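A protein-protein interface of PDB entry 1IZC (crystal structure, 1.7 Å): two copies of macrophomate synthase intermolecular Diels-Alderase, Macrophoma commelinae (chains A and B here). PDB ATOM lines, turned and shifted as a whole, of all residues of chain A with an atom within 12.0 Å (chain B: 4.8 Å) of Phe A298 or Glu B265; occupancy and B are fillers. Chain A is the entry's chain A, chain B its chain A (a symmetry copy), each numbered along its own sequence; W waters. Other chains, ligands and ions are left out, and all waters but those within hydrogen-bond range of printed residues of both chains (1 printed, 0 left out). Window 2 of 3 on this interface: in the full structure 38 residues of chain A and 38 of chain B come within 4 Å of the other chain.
O of Ser A294 is in hydrogen-bond range of NE2 of Gln A297 (2.9 Å).
O of Gln A290 is in hydrogen-bond range of OG of Ser A294 (3.4 Å).
OG of Ser A294 lies within hydrogen-bond range of O of Ala A291 (2.8 Å).
OD1 of Asp B38 lies within hydrogen-bond range of OG of Ser B40, 2.8 Å away.
Ser A294 touches Pro B261.
Ala A295 touches Ile B264 (CB to CD1, 3.7 Å).
Phe A298 touches Asp B38 (O to OD1, 3.8 Å).
CB of Phe A298 touches CB of Pro B39 (3.9 Å).
CB of Phe A298 touches N of Ser B40 (3.9 Å).
Phe A298 touches Pro B261.
Glu B265 touches Phe A298 (CG to CE1, 3.8 Å).
Ala A299 touches Asp B38 (CA to OD1, 3.5 Å).
Ala A299 touches Ser B40 (N to CB, 3.5 Å).
Gly A300 touches Asp B38 (N to OD1, 3.9 Å).
Ala A293 touches none of the printed residues of chain B.
Lys A296 touches none of the printed residues of chain B.
Of the printed residues of chain B, Gln A297 touches Pro B261.
Of the printed residues of chain B, Phe A298 touches Asp B38, Pro B39, Ser B40, Pro B261, Ile B264 and Glu B265.
Of the printed residues of chain B, Gly A300 touches Asp B38 (3.9 Å).
Asp B38 touches just these residues of chain A: Phe A298, Ala A299 and Gly A300.
Of chain A, only Ser A294 (3.8 Å), Gln A297 (3.6 Å) and Phe A298 (3.6 Å) come within 4 Å of Pro B261.
No residue of chain A comes within 4 Å of Ser B262.
Printed residues of chain A within 4 Å of Ile B264: Ala A295 (3.7 Å) and Phe A298 (3.8 Å).
Glu B265 touches just one residue of chain A: Phe A298 (3.8 Å).
Gln B266 touches none of the printed residues of chain A.
No residue of chain A comes within 4 Å of Gly B267.
The nearest residue of chain A that does not touch Glu B265 is Gln A297 (5.7 Å).
Of the 10 printed residues of chain B, 6 touch a printed residue of chain A.
Hydrophobic or aromatic side chains of chain A within 4 Å of the printed part of chain B: Ala A295, Phe A298 and Ala A299.
Among the printed residues, 13 pairs touch across the chains.
No position is printed for both chains.
Of the 13 pairs that touch across the chains among the printed residues, none has its exchanged pair printed and touching as well.
Water W1 lies within hydrogen-bond range of the backbone carbonyl oxygen of Ser B40 (2.8 Å) and the backbone carbonyl oxygen of Arg A292 (2.8 Å).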
ATOM      1  N   ALA A 289      -0.858   1.939 -21.691  1.00  0.00           N
ATOM      2  CA  ALA A 289      -0.238   1.552 -22.951  1.00  0.00           C
ATOM      3  C   ALA A 289       0.828   2.557 -23.373  1.00  0.00           C
ATOM      4  O   ALA A 289       1.935   2.170 -23.756  1.00  0.00           O
ATOM      5  CB  ALA A 289      -1.296   1.428 -24.047  1.00  0.00           C
ATOM      6  N   GLN A 290       0.495   3.844 -23.301  1.00  0.00           N
ATOM      7  CA  GLN A 290       1.431   4.884 -23.694  1.00  0.00           C
ATOM      8  C   GLN A 290       2.647   4.879 -22.784  1.00  0.00           C
ATOM      9  O   GLN A 290       3.785   5.015 -23.249  1.00  0.00           O
ATOM     10  CB  GLN A 290       0.764   6.254 -23.635  1.00  0.00           C
ATOM     11  CG  GLN A 290      -0.244   6.491 -24.735  1.00  0.00           C
ATOM     12  CD  GLN A 290      -1.015   7.779 -24.536  1.00  0.00           C
ATOM     13  OE1 GLN A 290      -0.457   8.789 -24.088  1.00  0.00           O
ATOM     14  NE2 GLN A 290      -2.303   7.760 -24.877  1.00  0.00           N
ATOM     15  N   ALA A 291       2.409   4.721 -21.484  1.00  0.00           N
ATOM     16  CA  ALA A 291       3.506   4.712 -20.525  1.00  0.00           C
ATOM     17  C   ALA A 291       4.470   3.553 -20.786  1.00  0.00           C
ATOM     18  O   ALA A 291       5.687   3.757 -20.862  1.00  0.00           O
ATOM     19  CB  ALA A 291       2.954   4.632 -19.090  1.00  0.00           C
ATOM     20  N   ARG A 292       3.935   2.343 -20.923  1.00  0.00           N
ATOM     21  CA  ARG A 292       4.780   1.177 -21.166  1.00  0.00           C
ATOM     22  C   ARG A 292       5.542   1.324 -22.476  1.00  0.00           C
ATOM     23  O   ARG A 292       6.733   0.997 -22.562  1.00  0.00           O
ATOM     24  CB  ARG A 292       3.945  -0.105 -21.203  1.00  0.00           C
ATOM     25  CG  ARG A 292       3.324  -0.479 -19.852  1.00  0.00           C
ATOM     26  CD  ARG A 292       2.814  -1.916 -19.865  1.00  0.00           C
ATOM     27  NE  ARG A 292       2.137  -2.281 -18.620  1.00  0.00           N
ATOM     28  CZ  ARG A 292       0.817  -2.365 -18.492  1.00  0.00           C
ATOM     29  NH1 ARG A 292       0.035  -2.110 -19.536  1.00  0.00           N
ATOM     30  NH2 ARG A 292       0.280  -2.704 -17.326  1.00  0.00           N
ATOM     31  N   ALA A 293       4.858   1.826 -23.497  1.00  0.00           N
ATOM     32  CA  ALA A 293       5.491   2.018 -24.796  1.00  0.00           C
ATOM     33  C   ALA A 293       6.673   2.977 -24.692  1.00  0.00           C
ATOM     34  O   ALA A 293       7.719   2.754 -25.303  1.00  0.00           O
ATOM     35  CB  ALA A 293       4.473   2.556 -25.797  1.00  0.00           C
ATOM     36  N   SER A 294       6.511   4.042 -23.912  1.00  0.00           N
ATOM     37  CA  SER A 294       7.556   5.040 -23.765  1.00  0.00           C
ATOM     38  C   SER A 294       8.718   4.548 -22.911  1.00  0.00           C
ATOM     39  O   SER A 294       9.797   5.147 -22.919  1.00  0.00           O
ATOM     40  CB  SER A 294       6.983   6.328 -23.171  1.00  0.00           C
ATOM     41  OG  SER A 294       6.685   6.185 -21.794  1.00  0.00           O
ATOM     42  N   ALA A 295       8.501   3.457 -22.182  1.00  0.00           N
ATOM     43  CA  ALA A 295       9.552   2.910 -21.327  1.00  0.00           C
ATOM     44  C   ALA A 295      10.422   1.901 -22.065  1.00  0.00           C
ATOM     45  O   ALA A 295      11.502   1.554 -21.601  1.00  0.00           O
ATOM     46  CB  ALA A 295       8.937   2.253 -20.094  1.00  0.00           C
ATOM     47  N   LYS A 296       9.954   1.424 -23.211  1.00  0.00           N
ATOM     48  CA  LYS A 296      10.705   0.436 -23.974  1.00  0.00           C
ATOM     49  C   LYS A 296      12.119   0.872 -24.346  1.00  0.00           C
ATOM     50  O   LYS A 296      12.996   0.027 -24.502  1.00  0.00           O
ATOM     51  CB  LYS A 296       9.940   0.047 -25.241  1.00  0.00           C
ATOM     52  CG  LYS A 296       8.796  -0.922 -24.990  1.00  0.00           C
ATOM     53  CD  LYS A 296       9.323  -2.278 -24.545  1.00  0.00           C
ATOM     54  CE  LYS A 296       8.203  -3.241 -24.188  1.00  0.00           C
ATOM     55  NZ  LYS A 296       7.319  -3.527 -25.347  1.00  0.00           N
ATOM     56  N   GLN A 297      12.337   2.179 -24.469  1.00  0.00           N
ATOM     57  CA  GLN A 297      13.648   2.717 -24.840  1.00  0.00           C
ATOM     58  C   GLN A 297      14.716   2.463 -23.779  1.00  0.00           C
ATOM     59  O   GLN A 297      15.916   2.631 -24.036  1.00  0.00           O
ATOM     60  CB  GLN A 297      13.537   4.221 -25.092  1.00  0.00           C
ATOM     61  CG  GLN A 297      13.095   5.001 -23.865  1.00  0.00           C
ATOM     62  CD  GLN A 297      12.940   6.487 -24.118  1.00  0.00           C
ATOM     63  OE1 GLN A 297      13.912   7.188 -24.408  1.00  0.00           O
ATOM     64  NE2 GLN A 297      11.712   6.980 -24.003  1.00  0.00           N
ATOM     65  N   PHE A 298      14.285   2.052 -22.590  1.00  0.00           N
ATOM     66  CA  PHE A 298      15.215   1.793 -21.500  1.00  0.00           C
ATOM     67  C   PHE A 298      15.583   0.322 -21.351  1.00  0.00           C
ATOM     68  O   PHE A 298      16.337  -0.042 -20.447  1.00  0.00           O
ATOM     69  CB  PHE A 298      14.618   2.316 -20.191  1.00  0.00           C
ATOM     70  CG  PHE A 298      14.366   3.787 -20.198  1.00  0.00           C
ATOM     71  CD1 PHE A 298      15.421   4.684 -20.069  1.00  0.00           C
ATOM     72  CD2 PHE A 298      13.076   4.285 -20.364  1.00  0.00           C
ATOM     73  CE1 PHE A 298      15.200   6.047 -20.104  1.00  0.00           C
ATOM     74  CE2 PHE A 298      12.844   5.653 -20.401  1.00  0.00           C
ATOM     75  CZ  PHE A 298      13.908   6.538 -20.270  1.00  0.00           C
ATOM     76  N   ALA A 299      15.059  -0.517 -22.237  1.00  0.00           N
ATOM     77  CA  ALA A 299      15.327  -1.948 -22.198  1.00  0.00           C
ATOM     78  C   ALA A 299      16.820  -2.229 -22.318  1.00  0.00           C
ATOM     79  O   ALA A 299      17.563  -1.457 -22.929  1.00  0.00           O
ATOM     80  CB  ALA A 299      14.577  -2.652 -23.308  1.00  0.00           C
ATOM     81  N   GLY A 300      17.238  -3.345 -21.732  1.00  0.00           N
ATOM     82  CA  GLY A 300      18.636  -3.729 -21.742  1.00  0.00           C
ATOM     83  C   GLY A 300      19.280  -3.354 -20.416  1.00  0.00           C
ATOM     84  O   GLY A 300      20.364  -2.724 -20.442  1.00  0.00           O
ATOM     85  N   ASP B  38      15.977  -3.607 -15.088  1.00  0.00           N
ATOM     86  CA  ASP B  38      15.572  -3.269 -16.451  1.00  0.00           C
ATOM     87  C   ASP B  38      14.455  -2.236 -16.353  1.00  0.00           C
ATOM     88  O   ASP B  38      13.292  -2.594 -16.222  1.00  0.00           O
ATOM     89  CB  ASP B  38      15.070  -4.526 -17.165  1.00  0.00           C
ATOM     90  CG  ASP B  38      14.593  -4.248 -18.582  1.00  0.00           C
ATOM     91  OD1 ASP B  38      14.548  -3.067 -18.970  1.00  0.00           O
ATOM     92  OD2 ASP B  38      14.266  -5.221 -19.296  1.00  0.00           O
ATOM     93  N   PRO B  39      14.804  -0.940 -16.419  1.00  0.00           N
ATOM     94  CA  PRO B  39      13.828   0.151 -16.326  1.00  0.00           C
ATOM     95  C   PRO B  39      12.690   0.156 -17.340  1.00  0.00           C
ATOM     96  O   PRO B  39      11.735   0.913 -17.172  1.00  0.00           O
ATOM     97  CB  PRO B  39      14.696   1.405 -16.404  1.00  0.00           C
ATOM     98  CG  PRO B  39      15.995   0.933 -15.776  1.00  0.00           C
ATOM     99  CD  PRO B  39      16.177  -0.408 -16.434  1.00  0.00           C
ATOM    100  N   SER B  40      12.785  -0.663 -18.387  1.00  0.00           N
ATOM    101  CA  SER B  40      11.689  -0.723 -19.350  1.00  0.00           C
ATOM    102  C   SER B  40      10.542  -1.445 -18.644  1.00  0.00           C
ATOM    103  O   SER B  40       9.398  -1.434 -19.116  1.00  0.00           O
ATOM    104  CB  SER B  40      12.094  -1.487 -20.621  1.00  0.00           C
ATOM    105  OG  SER B  40      12.197  -2.885 -20.402  1.00  0.00           O
ATOM    106  N   PRO B 261       9.250   9.087 -19.499  1.00  0.00           N
ATOM    107  CA  PRO B 261      10.684   8.894 -19.755  1.00  0.00           C
ATOM    108  C   PRO B 261      11.572   9.677 -18.801  1.00  0.00           C
ATOM    109  O   PRO B 261      12.549   9.149 -18.271  1.00  0.00           O
ATOM    110  CB  PRO B 261      10.839   9.354 -21.202  1.00  0.00           C
ATOM    111  CG  PRO B 261       9.543   8.907 -21.810  1.00  0.00           C
ATOM    112  CD  PRO B 261       8.530   9.358 -20.757  1.00  0.00           C
ATOM    113  N   SER B 262      11.228  10.935 -18.570  1.00  0.00           N
ATOM    114  CA  SER B 262      12.012  11.773 -17.678  1.00  0.00           C
ATOM    115  C   SER B 262      11.975  11.219 -16.254  1.00  0.00           C
ATOM    116  O   SER B 262      12.989  11.213 -15.549  1.00  0.00           O
ATOM    117  CB  SER B 262      11.476  13.204 -17.686  1.00  0.00           C
ATOM    118  OG  SER B 262      12.263  14.029 -16.841  1.00  0.00           O
ATOM    119  N   LEU B 263      10.804  10.750 -15.825  1.00  0.00           N
ATOM    120  CA  LEU B 263      10.699  10.201 -14.477  1.00  0.00           C
ATOM    121  C   LEU B 263      11.570   8.960 -14.349  1.00  0.00           C
ATOM    122  O   LEU B 263      12.230   8.768 -13.332  1.00  0.00           O
ATOM    123  CB  LEU B 263       9.236   9.864 -14.144  1.00  0.00           C
ATOM    124  CG  LEU B 263       8.314  11.088 -14.106  1.00  0.00           C
ATOM    125  CD1 LEU B 263       6.861  10.648 -13.957  1.00  0.00           C
ATOM    126  CD2 LEU B 263       8.723  12.006 -12.953  1.00  0.00           C
ATOM    127  N   ILE B 264      11.581   8.114 -15.376  1.00  0.00           N
ATOM    128  CA  ILE B 264      12.399   6.910 -15.320  1.00  0.00           C
ATOM    129  C   ILE B 264      13.873   7.299 -15.242  1.00  0.00           C
ATOM    130  O   ILE B 264      14.643   6.690 -14.498  1.00  0.00           O
ATOM    131  CB  ILE B 264      12.154   6.000 -16.546  1.00  0.00           C
ATOM    132  CG1 ILE B 264      10.752   5.370 -16.434  1.00  0.00           C
ATOM    133  CG2 ILE B 264      13.226   4.898 -16.620  1.00  0.00           C
ATOM    134  CD1 ILE B 264      10.298   4.641 -17.672  1.00  0.00           C
ATOM    135  N   GLU B 265      14.259   8.329 -15.987  1.00  0.00           N
ATOM    136  CA  GLU B 265      15.653   8.783 -15.983  1.00  0.00           C
ATOM    137  C   GLU B 265      16.033   9.301 -14.604  1.00  0.00           C
ATOM    138  O   GLU B 265      17.196   9.227 -14.194  1.00  0.00           O
ATOM    139  CB  GLU B 265      15.862   9.891 -17.023  1.00  0.00           C
ATOM    140  CG  GLU B 265      15.610   9.439 -18.449  1.00  0.00           C
ATOM    141  CD  GLU B 265      15.743  10.567 -19.462  1.00  0.00           C
ATOM    142  OE1 GLU B 265      15.098  11.625 -19.275  1.00  0.00           O
ATOM    143  OE2 GLU B 265      16.490  10.391 -20.449  1.00  0.00           O
ATOM    144  N   GLN B 266      15.041   9.820 -13.894  1.00  0.00           N
ATOM    145  CA  GLN B 266      15.235  10.356 -12.554  1.00  0.00           C
ATOM    146  C   GLN B 266      15.244   9.282 -11.469  1.00  0.00           C
ATOM    147  O   GLN B 266      15.490   9.580 -10.301  1.00  0.00           O
ATOM    148  CB  GLN B 266      14.143  11.369 -12.235  1.00  0.00           C
ATOM    149  CG  GLN B 266      14.210  12.629 -13.057  1.00  0.00           C
ATOM    150  CD  GLN B 266      13.064  13.562 -12.749  1.00  0.00           C
ATOM    151  OE1 GLN B 266      12.860  13.953 -11.596  1.00  0.00           O
ATOM    152  NE2 GLN B 266      12.304  13.927 -13.776  1.00  0.00           N
ATOM    153  N   GLY B 267      14.958   8.041 -11.849  1.00  0.00           N
ATOM    154  CA  GLY B 267      14.965   6.968 -10.874  1.00  0.00           C
ATOM    155  C   GLY B 267      13.607   6.424 -10.461  1.00  0.00           C
ATOM    156  O   GLY B 267      13.542   5.580  -9.572  1.00  0.00           O
HETATM  157  O   HOH W   1       8.230  -1.195 -21.616  1.00  0.00           O
